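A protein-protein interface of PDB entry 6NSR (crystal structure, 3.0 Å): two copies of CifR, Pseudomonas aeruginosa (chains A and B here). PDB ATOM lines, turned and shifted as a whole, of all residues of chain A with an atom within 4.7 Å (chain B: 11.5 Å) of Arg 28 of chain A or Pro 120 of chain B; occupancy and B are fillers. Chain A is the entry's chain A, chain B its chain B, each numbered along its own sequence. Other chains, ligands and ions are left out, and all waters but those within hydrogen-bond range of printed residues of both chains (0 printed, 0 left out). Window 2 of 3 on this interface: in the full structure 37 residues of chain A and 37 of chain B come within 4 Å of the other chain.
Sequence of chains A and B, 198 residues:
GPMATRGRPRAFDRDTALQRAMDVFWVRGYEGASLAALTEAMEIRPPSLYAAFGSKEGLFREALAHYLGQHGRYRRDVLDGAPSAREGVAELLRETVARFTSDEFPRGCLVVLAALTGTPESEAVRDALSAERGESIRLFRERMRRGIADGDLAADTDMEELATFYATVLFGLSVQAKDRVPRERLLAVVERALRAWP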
ATOM      1  N   VAL A  24      10.344 -17.725  30.222  1.00  0.00           N
ATOM      2  CA  VAL A  24      11.007 -19.025  30.307  1.00  0.00           C
ATOM      3  C   VAL A  24      10.319 -20.038  29.401  1.00  0.00           C
ATOM      4  O   VAL A  24      10.978 -20.803  28.686  1.00  0.00           O
ATOM      5  CB  VAL A  24      11.064 -19.504  31.769  1.00  0.00           C
ATOM      6  CG1 VAL A  24      11.729 -20.866  31.852  1.00  0.00           C
ATOM      7  CG2 VAL A  24      11.799 -18.494  32.622  1.00  0.00           C
ATOM      8  N   PHE A  25       8.985 -20.058  29.418  1.00  0.00           N
ATOM      9  CA  PHE A  25       8.238 -20.930  28.517  1.00  0.00           C
ATOM     10  C   PHE A  25       8.509 -20.568  27.062  1.00  0.00           C
ATOM     11  O   PHE A  25       8.778 -21.443  26.231  1.00  0.00           O
ATOM     12  CB  PHE A  25       6.744 -20.827  28.822  1.00  0.00           C
ATOM     13  CG  PHE A  25       6.323 -21.550  30.071  1.00  0.00           C
ATOM     14  CD1 PHE A  25       6.741 -22.848  30.314  1.00  0.00           C
ATOM     15  CD2 PHE A  25       5.514 -20.926  31.007  1.00  0.00           C
ATOM     16  CE1 PHE A  25       6.353 -23.512  31.464  1.00  0.00           C
ATOM     17  CE2 PHE A  25       5.126 -21.584  32.158  1.00  0.00           C
ATOM     18  CZ  PHE A  25       5.546 -22.878  32.387  1.00  0.00           C
ATOM     19  N   TRP A  26       8.403 -19.276  26.734  1.00  0.00           N
ATOM     20  CA  TRP A  26       8.664 -18.798  25.378  1.00  0.00           C
ATOM     21  C   TRP A  26       9.980 -19.322  24.812  1.00  0.00           C
ATOM     22  O   TRP A  26      10.069 -19.639  23.620  1.00  0.00           O
ATOM     23  CB  TRP A  26       8.674 -17.269  25.380  1.00  0.00           C
ATOM     24  CG  TRP A  26       8.224 -16.644  24.099  1.00  0.00           C
ATOM     25  CD1 TRP A  26       8.143 -17.242  22.876  1.00  0.00           C
ATOM     26  CD2 TRP A  26       7.797 -15.290  23.912  1.00  0.00           C
ATOM     27  NE1 TRP A  26       7.689 -16.346  21.939  1.00  0.00           N
ATOM     28  CE2 TRP A  26       7.469 -15.140  22.551  1.00  0.00           C
ATOM     29  CE3 TRP A  26       7.657 -14.191  24.765  1.00  0.00           C
ATOM     30  CZ2 TRP A  26       7.011 -13.935  22.022  1.00  0.00           C
ATOM     31  CZ3 TRP A  26       7.204 -12.997  24.239  1.00  0.00           C
ATOM     32  CH2 TRP A  26       6.887 -12.878  22.881  1.00  0.00           C
ATOM     33  N   VAL A  27      10.979 -19.488  25.646  1.00  0.00           N
ATOM     34  CA  VAL A  27      12.250 -19.958  25.151  1.00  0.00           C
ATOM     35  C   VAL A  27      12.487 -21.447  25.297  1.00  0.00           C
ATOM     36  O   VAL A  27      13.038 -22.063  24.421  1.00  0.00           O
ATOM     37  CB  VAL A  27      13.385 -19.228  25.839  1.00  0.00           C
ATOM     38  CG1 VAL A  27      14.681 -19.541  25.146  1.00  0.00           C
ATOM     39  CG2 VAL A  27      13.138 -17.744  25.802  1.00  0.00           C
ATOM     40  N   ARG A  28      12.101 -22.061  26.395  1.00  0.00           N
ATOM     41  CA  ARG A  28      12.416 -23.464  26.549  1.00  0.00           C
ATOM     42  C   ARG A  28      11.267 -24.358  26.269  1.00  0.00           C
ATOM     43  O   ARG A  28      11.415 -25.548  26.178  1.00  0.00           O
ATOM     44  CB  ARG A  28      12.849 -23.748  27.949  1.00  0.00           C
ATOM     45  CG  ARG A  28      13.707 -22.686  28.532  1.00  0.00           C
ATOM     46  CD  ARG A  28      14.590 -23.321  29.547  1.00  0.00           C
ATOM     47  NE  ARG A  28      15.679 -22.443  29.875  1.00  0.00           N
ATOM     48  CZ  ARG A  28      16.527 -22.693  30.848  1.00  0.00           C
ATOM     49  NH1 ARG A  28      16.374 -23.793  31.559  1.00  0.00           N
ATOM     50  NH2 ARG A  28      17.513 -21.852  31.103  1.00  0.00           N
ATOM     51  N   GLY A  29      10.097 -23.797  26.160  1.00  0.00           N
ATOM     52  CA  GLY A  29       8.948 -24.624  25.880  1.00  0.00           C
ATOM     53  C   GLY A  29       8.268 -25.047  27.152  1.00  0.00           C
ATOM     54  O   GLY A  29       8.814 -24.871  28.206  1.00  0.00           O
ATOM     55  N   TYR A  30       7.080 -25.614  27.071  1.00  0.00           N
ATOM     56  CA  TYR A  30       6.447 -26.034  28.275  1.00  0.00           C
ATOM     57  C   TYR A  30       7.281 -27.044  29.006  1.00  0.00           C
ATOM     58  O   TYR A  30       7.569 -26.877  30.164  1.00  0.00           O
ATOM     59  CB  TYR A  30       5.086 -26.605  27.968  1.00  0.00           C
ATOM     60  CG  TYR A  30       4.441 -27.238  29.135  1.00  0.00           C
ATOM     61  CD1 TYR A  30       4.110 -26.509  30.237  1.00  0.00           C
ATOM     62  CD2 TYR A  30       4.194 -28.566  29.144  1.00  0.00           C
ATOM     63  CE1 TYR A  30       3.522 -27.098  31.319  1.00  0.00           C
ATOM     64  CE2 TYR A  30       3.607 -29.166  30.213  1.00  0.00           C
ATOM     65  CZ  TYR A  30       3.274 -28.429  31.296  1.00  0.00           C
ATOM     66  OH  TYR A  30       2.693 -29.069  32.344  1.00  0.00           O
ATOM     67  N   GLY A  32      10.464 -28.089  28.414  1.00  0.00           N
ATOM     68  CA  GLY A  32      11.849 -27.700  28.609  1.00  0.00           C
ATOM     69  C   GLY A  32      12.054 -26.756  29.774  1.00  0.00           C
ATOM     70  O   GLY A  32      13.161 -26.685  30.319  1.00  0.00           O
ATOM     71  N   ALA A  33      11.015 -26.021  30.161  1.00  0.00           N
ATOM     72  CA  ALA A  33      11.105 -25.075  31.265  1.00  0.00           C
ATOM     73  C   ALA A  33      10.926 -25.854  32.561  1.00  0.00           C
ATOM     74  O   ALA A  33       9.807 -26.251  32.903  1.00  0.00           O
ATOM     75  CB  ALA A  33      10.028 -24.004  31.122  1.00  0.00           C
ATOM     76  N   ALA A  37      14.442 -23.615  36.644  1.00  0.00           N
ATOM     77  CA  ALA A  37      14.592 -22.444  35.788  1.00  0.00           C
ATOM     78  C   ALA A  37      13.452 -21.453  35.986  1.00  0.00           C
ATOM     79  O   ALA A  37      13.666 -20.238  35.915  1.00  0.00           O
ATOM     80  CB  ALA A  37      14.669 -22.871  34.324  1.00  0.00           C
ATOM     81  N   ARG B  28       7.187 -37.989  19.980  1.00  0.00           N
ATOM     82  CA  ARG B  28       7.497 -37.325  21.238  1.00  0.00           C
ATOM     83  C   ARG B  28       8.591 -36.271  21.145  1.00  0.00           C
ATOM     84  O   ARG B  28       8.804 -35.545  22.123  1.00  0.00           O
ATOM     85  CB  ARG B  28       7.906 -38.357  22.299  1.00  0.00           C
ATOM     86  CG  ARG B  28       6.863 -39.416  22.597  1.00  0.00           C
ATOM     87  CD  ARG B  28       7.243 -40.199  23.840  1.00  0.00           C
ATOM     88  NE  ARG B  28       6.258 -41.221  24.179  1.00  0.00           N
ATOM     89  CZ  ARG B  28       6.214 -41.857  25.342  1.00  0.00           C
ATOM     90  NH1 ARG B  28       7.081 -41.593  26.307  1.00  0.00           N
ATOM     91  NH2 ARG B  28       5.278 -42.780  25.542  1.00  0.00           N
ATOM     92  N   TYR B  30      12.719 -35.012  20.592  1.00  0.00           N
ATOM     93  CA  TYR B  30      14.009 -35.495  21.079  1.00  0.00           C
ATOM     94  C   TYR B  30      14.002 -35.682  22.590  1.00  0.00           C
ATOM     95  O   TYR B  30      14.203 -36.794  23.090  1.00  0.00           O
ATOM     96  CB  TYR B  30      15.135 -34.545  20.669  1.00  0.00           C
ATOM     97  CG  TYR B  30      16.450 -34.895  21.331  1.00  0.00           C
ATOM     98  CD1 TYR B  30      17.173 -36.014  20.939  1.00  0.00           C
ATOM     99  CD2 TYR B  30      16.960 -34.115  22.361  1.00  0.00           C
ATOM    100  CE1 TYR B  30      18.371 -36.340  21.547  1.00  0.00           C
ATOM    101  CE2 TYR B  30      18.156 -34.434  22.975  1.00  0.00           C
ATOM    102  CZ  TYR B  30      18.857 -35.547  22.564  1.00  0.00           C
ATOM    103  OH  TYR B  30      20.048 -35.869  23.171  1.00  0.00           O
ATOM    104  N   GLU B  31      13.753 -34.607  23.339  1.00  0.00           N
ATOM    105  CA  GLU B  31      13.777 -34.720  24.792  1.00  0.00           C
ATOM    106  C   GLU B  31      12.517 -35.374  25.343  1.00  0.00           C
ATOM    107  O   GLU B  31      12.562 -35.989  26.414  1.00  0.00           O
ATOM    108  CB  GLU B  31      14.059 -33.369  25.453  1.00  0.00           C
ATOM    109  CG  GLU B  31      13.008 -32.302  25.229  1.00  0.00           C
ATOM    110  CD  GLU B  31      13.406 -30.973  25.846  1.00  0.00           C
ATOM    111  OE1 GLU B  31      14.598 -30.805  26.181  1.00  0.00           O
ATOM    112  OE2 GLU B  31      12.523 -30.102  26.005  1.00  0.00           O
ATOM    113  N   GLY B  32      11.394 -35.267  24.630  1.00  0.00           N
ATOM    114  CA  GLY B  32      10.171 -35.895  25.092  1.00  0.00           C
ATOM    115  C   GLY B  32      10.199 -37.407  25.022  1.00  0.00           C
ATOM    116  O   GLY B  32       9.434 -38.066  25.735  1.00  0.00           O
ATOM    117  N   GLU B  57      21.708 -38.748  22.418  1.00  0.00           N
ATOM    118  CA  GLU B  57      21.943 -37.832  21.307  1.00  0.00           C
ATOM    119  C   GLU B  57      22.479 -38.574  20.090  1.00  0.00           C
ATOM    120  O   GLU B  57      22.091 -38.281  18.953  1.00  0.00           O
ATOM    121  CB  GLU B  57      22.902 -36.720  21.729  1.00  0.00           C
ATOM    122  CG  GLU B  57      23.301 -35.790  20.595  1.00  0.00           C
ATOM    123  CD  GLU B  57      24.158 -34.632  21.063  1.00  0.00           C
ATOM    124  OE1 GLU B  57      24.061 -34.262  22.251  1.00  0.00           O
ATOM    125  OE2 GLU B  57      24.928 -34.092  20.240  1.00  0.00           O
ATOM    126  N   ARG B  61      20.815 -38.841  16.351  1.00  0.00           N
ATOM    127  CA  ARG B  61      21.525 -38.524  15.118  1.00  0.00           C
ATOM    128  C   ARG B  61      21.441 -39.675  14.122  1.00  0.00           C
ATOM    129  O   ARG B  61      21.247 -39.451  12.922  1.00  0.00           O
ATOM    130  CB  ARG B  61      22.973 -38.153  15.427  1.00  0.00           C
ATOM    131  CG  ARG B  61      23.099 -36.843  16.182  1.00  0.00           C
ATOM    132  CD  ARG B  61      24.545 -36.429  16.359  1.00  0.00           C
ATOM    133  NE  ARG B  61      24.654 -35.152  17.054  1.00  0.00           N
ATOM    134  CZ  ARG B  61      24.580 -33.970  16.461  1.00  0.00           C
ATOM    135  NH1 ARG B  61      24.381 -33.862  15.156  1.00  0.00           N
ATOM    136  NH2 ARG B  61      24.704 -32.866  17.195  1.00  0.00           N
ATOM    137  N   LEU B 113       9.093 -30.958  13.945  1.00  0.00           N
ATOM    138  CA  LEU B 113       8.368 -31.233  15.180  1.00  0.00           C
ATOM    139  C   LEU B 113       9.248 -31.735  16.317  1.00  0.00           C
ATOM    140  O   LEU B 113       8.852 -31.609  17.482  1.00  0.00           O
ATOM    141  CB  LEU B 113       7.266 -32.267  14.927  1.00  0.00           C
ATOM    142  CG  LEU B 113       6.242 -31.959  13.835  1.00  0.00           C
ATOM    143  CD1 LEU B 113       5.304 -33.140  13.642  1.00  0.00           C
ATOM    144  CD2 LEU B 113       5.461 -30.701  14.176  1.00  0.00           C
ATOM    145  N   ALA B 114      10.423 -32.294  16.018  1.00  0.00           N
ATOM    146  CA  ALA B 114      11.185 -33.006  17.041  1.00  0.00           C
ATOM    147  C   ALA B 114      11.704 -32.069  18.128  1.00  0.00           C
ATOM    148  O   ALA B 114      11.578 -32.367  19.322  1.00  0.00           O
ATOM    149  CB  ALA B 114      12.331 -33.796  16.406  1.00  0.00           C
ATOM    150  N   ALA B 115      12.304 -30.939  17.745  1.00  0.00           N
ATOM    151  CA  ALA B 115      12.884 -30.043  18.752  1.00  0.00           C
ATOM    152  C   ALA B 115      12.952 -28.615  18.200  1.00  0.00           C
ATOM    153  O   ALA B 115      13.928 -28.241  17.549  1.00  0.00           O
ATOM    154  CB  ALA B 115      14.245 -30.524  19.216  1.00  0.00           C
ATOM    155  N   LEU B 116      11.911 -27.831  18.478  1.00  0.00           N
ATOM    156  CA  LEU B 116      11.959 -26.397  18.214  1.00  0.00           C
ATOM    157  C   LEU B 116      12.434 -25.611  19.430  1.00  0.00           C
ATOM    158  O   LEU B 116      13.175 -24.633  19.288  1.00  0.00           O
ATOM    159  CB  LEU B 116      10.590 -25.885  17.758  1.00  0.00           C
ATOM    160  CG  LEU B 116      10.191 -26.233  16.325  1.00  0.00           C
ATOM    161  CD1 LEU B 116       8.838 -25.633  15.980  1.00  0.00           C
ATOM    162  CD2 LEU B 116      11.253 -25.764  15.346  1.00  0.00           C
ATOM    163  N   THR B 117      12.009 -26.019  20.623  1.00  0.00           N
ATOM    164  CA  THR B 117      12.452 -25.447  21.885  1.00  0.00           C
ATOM    165  C   THR B 117      12.916 -26.583  22.789  1.00  0.00           C
ATOM    166  O   THR B 117      12.866 -27.759  22.416  1.00  0.00           O
ATOM    167  CB  THR B 117      11.333 -24.634  22.547  1.00  0.00           C
ATOM    168  OG1 THR B 117      10.123 -25.401  22.556  1.00  0.00           O
ATOM    169  CG2 THR B 117      11.098 -23.334  21.791  1.00  0.00           C
ATOM    170  N   GLY B 118      13.374 -26.232  23.980  1.00  0.00           N
ATOM    171  CA  GLY B 118      13.811 -27.226  24.935  1.00  0.00           C
ATOM    172  C   GLY B 118      14.848 -26.658  25.883  1.00  0.00           C
ATOM    173  O   GLY B 118      15.116 -25.461  25.899  1.00  0.00           O
ATOM    174  N   THR B 119      15.419 -27.561  26.678  1.00  0.00           N
ATOM    175  CA  THR B 119      16.439 -27.193  27.645  1.00  0.00           C
ATOM    176  C   THR B 119      17.731 -26.797  26.931  1.00  0.00           C
ATOM    177  O   THR B 119      17.980 -27.223  25.800  1.00  0.00           O
ATOM    178  CB  THR B 119      16.721 -28.375  28.565  1.00  0.00           C
ATOM    179  OG1 THR B 119      17.309 -29.438  27.807  1.00  0.00           O
ATOM    180  CG2 THR B 119      15.431 -28.871  29.196  1.00  0.00           C
ATOM    181  N   PRO B 120      18.567 -25.969  27.568  1.00  0.00           N
ATOM    182  CA  PRO B 120      19.877 -25.657  26.971  1.00  0.00           C
ATOM    183  C   PRO B 120      20.723 -26.888  26.705  1.00  0.00           C
ATOM    184  O   PRO B 120      21.502 -26.897  25.744  1.00  0.00           O
ATOM    185  CB  PRO B 120      20.529 -24.734  28.008  1.00  0.00           C
ATOM    186  CG  PRO B 120      19.389 -24.147  28.764  1.00  0.00           C
ATOM    187  CD  PRO B 120      18.330 -25.211  28.809  1.00  0.00           C
ATOM    188  N   GLU B 121      20.606 -27.922  27.544  1.00  0.00           N
ATOM    189  CA  GLU B 121      21.423 -29.122  27.399  1.00  0.00           C
ATOM    190  C   GLU B 121      21.271 -29.773  26.029  1.00  0.00           C
ATOM    191  O   GLU B 121      22.184 -30.474  25.583  1.00  0.00           O
ATOM    192  CB  GLU B 121      21.090 -30.123  28.507  1.00  0.00           C
ATOM    193  CG  GLU B 121      21.377 -29.609  29.913  1.00  0.00           C
ATOM    194  CD  GLU B 121      20.185 -28.907  30.535  1.00  0.00           C
ATOM    195  OE1 GLU B 121      19.092 -29.510  30.579  1.00  0.00           O
ATOM    196  OE2 GLU B 121      20.341 -27.749  30.980  1.00  0.00           O
ATOM    197  N   SER B 122      20.146 -29.551  25.350  1.00  0.00           N
ATOM    198  CA  SER B 122      19.870 -30.166  24.060  1.00  0.00           C
ATOM    199  C   SER B 122      20.138 -29.234  22.884  1.00  0.00           C
ATOM    200  O   SER B 122      19.717 -29.540  21.763  1.00  0.00           O
ATOM    201  CB  SER B 122      18.429 -30.682  24.011  1.00  0.00           C
ATOM    202  OG  SER B 122      17.503 -29.613  24.084  1.00  0.00           O
ATOM    203  N   GLU B 123      20.776 -28.085  23.124  1.00  0.00           N
ATOM    204  CA  GLU B 123      21.079 -27.098  22.090  1.00  0.00           C
ATOM    205  C   GLU B 123      21.598 -27.722  20.799  1.00  0.00           C
ATOM    206  O   GLU B 123      21.184 -27.325  19.704  1.00  0.00           O
ATOM    207  CB  GLU B 123      22.088 -26.070  22.606  1.00  0.00           C
ATOM    208  CG  GLU B 123      21.459 -24.811  23.173  1.00  0.00           C
ATOM    209  CD  GLU B 123      22.318 -23.584  22.947  1.00  0.00           C
ATOM    210  OE1 GLU B 123      22.948 -23.489  21.872  1.00  0.00           O
ATOM    211  OE2 GLU B 123      22.370 -22.720  23.847  1.00  0.00           O
ATOM    212  N   ALA B 124      22.516 -28.687  20.923  1.00  0.00           N
ATOM    213  CA  ALA B 124      23.075 -29.368  19.759  1.00  0.00           C
ATOM    214  C   ALA B 124      21.976 -29.922  18.858  1.00  0.00           C
ATOM    215  O   ALA B 124      21.907 -29.599  17.666  1.00  0.00           O
ATOM    216  CB  ALA B 124      24.018 -30.483  20.216  1.00  0.00           C
ATOM    217  N   VAL B 125      21.134 -30.798  19.414  1.00  0.00           N
ATOM    218  CA  VAL B 125      20.061 -31.428  18.645  1.00  0.00           C
ATOM    219  C   VAL B 125      19.257 -30.382  17.880  1.00  0.00           C
ATOM    220  O   VAL B 125      19.061 -30.491  16.663  1.00  0.00           O
ATOM    221  CB  VAL B 125      19.170 -32.286  19.561  1.00  0.00           C
ATOM    222  CG1 VAL B 125      17.879 -32.659  18.850  1.00  0.00           C
ATOM    223  CG2 VAL B 125      19.922 -33.529  20.000  1.00  0.00           C
ATOM    224  N   ARG B 126      18.748 -29.375  18.595  1.00  0.00           N
ATOM    225  CA  ARG B 126      17.976 -28.308  17.962  1.00  0.00           C
ATOM    226  C   ARG B 126      18.724 -27.708  16.777  1.00  0.00           C
ATOM    227  O   ARG B 126      18.187 -27.621  15.666  1.00  0.00           O
ATOM    228  CB  ARG B 126      17.608 -27.235  18.989  1.00  0.00           C
ATOM    229  CG  ARG B 126      16.540 -27.675  19.975  1.00  0.00           C
ATOM    230  CD  ARG B 126      15.920 -26.484  20.681  1.00  0.00           C
ATOM    231  NE  ARG B 126      16.908 -25.691  21.402  1.00  0.00           N
ATOM    232  CZ  ARG B 126      17.290 -25.925  22.649  1.00  0.00           C
ATOM    233  NH1 ARG B 126      16.783 -26.925  23.350  1.00  0.00           N
ATOM    234  NH2 ARG B 126      18.200 -25.133  23.208  1.00  0.00           N
ATOM    235  N   ASP B 127      19.956 -27.248  17.012  1.00  0.00           N
ATOM    236  CA  ASP B 127      20.747 -26.649  15.939  1.00  0.00           C
ATOM    237  C   ASP B 127      20.875 -27.592  14.748  1.00  0.00           C
ATOM    238  O   ASP B 127      20.794 -27.160  13.593  1.00  0.00           O
ATOM    239  CB  ASP B 127      22.125 -26.244  16.465  1.00  0.00           C
ATOM    240  CG  ASP B 127      22.056 -25.076  17.428  1.00  0.00           C
ATOM    241  OD1 ASP B 127      20.950 -24.519  17.602  1.00  0.00           O
ATOM    242  OD2 ASP B 127      23.101 -24.719  18.014  1.00  0.00           O
ATOM    243  N   ALA B 128      21.116 -28.879  15.015  1.00  0.00           N
ATOM    244  CA  ALA B 128      21.165 -29.878  13.950  1.00  0.00           C
ATOM    245  C   ALA B 128      19.913 -29.809  13.083  1.00  0.00           C
ATOM    246  O   ALA B 128      19.991 -29.672  11.857  1.00  0.00           O
ATOM    247  CB  ALA B 128      21.342 -31.275  14.549  1.00  0.00           C
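The backbone NH (N) of Gly 118 of chain B sits at hydrogen-bond distance from the backbone carbonyl oxygen (O) of Arg 28 of chain A, 3.0 Å away.
The backbone carbonyl oxygen (O) of Gly 118 of chain B lies close to the guanidinium group (NH1) of Arg 126 of chain B, at 3.4 Å.
O of Thr 119 of chain B is in hydrogen-bond range of OG of Ser 122 of chain B, at 3.0 Å.
The side-chain carboxylate of Glu 31 of chain B sits at hydrogen-bond distance from the backbone NH of Thr 119 of chain B (3.4 Å).
The guanidinium group (NH1) of Arg 126 of chain B is in hydrogen-bond range of the backbone carbonyl oxygen (O) of Thr 119 of chain B, 2.7 Å away.
OG1 of Thr 119 of chain B sits at hydrogen-bond distance from OE1 of Glu 121 of chain B (3.3 Å).
Among the printed residues, pairs that only touch across the chains: Gly 32 of chain A with Thr 119 of chain B (3.3 Å), Val 27 of chain A with Thr 117 of chain B (3.5 Å), Gly 32 of chain A with Glu 31 of chain B (3.6 Å), Gly 29 of chain A with Thr 117 of chain B (3.6 Å), Arg 28 of chain A with Pro 120 of chain B (3.7 Å) and Arg 28 of chain A with Thr 117 of chain B (3.7 Å).
Arg 28 of chain A touches just these residues of chain B: Thr 117 (3.7 Å), Gly 118 (3.0 Å) and Pro 120 (3.7 Å).
Pro 120 of chain B touches one residue of chain A.
No residue of chain B comes within 4 Å of Val 24 of chain A.
Of the printed residues of chain B, Val 27 of chain A touches Thr 117.
Gly 29 of chain A touches just one residue of chain B: Thr 117.
No residue of chain B comes within 4 Å of Ala 33 of chain A.
No residue of chain B comes within 4 Å of Ala 37 of chain A.
Printed residues of chain A within 4 Å of Thr 119 of chain B: Gly 32.
Of the printed residues of chain A, Thr 117 of chain B touches Val 27, Arg 28 and Gly 29.
The nearest printed residue of chain A that does not touch Glu 31 of chain B is Arg 28 of chain A (4.7 Å).
Of the 10 printed residues of chain A, 4 touch a printed residue of chain B.
Among the printed residues, 7 pairs touch across the chains.
Among the printed residues, no Asp or Glu carboxylate lies within 4 Å of a Lys or Arg side-chain nitrogen of the other chain.
3 positions are printed for both chains.
Of the 7 pairs that touch across the chains among the printed residues, none has its exchanged pair printed and touching as well.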
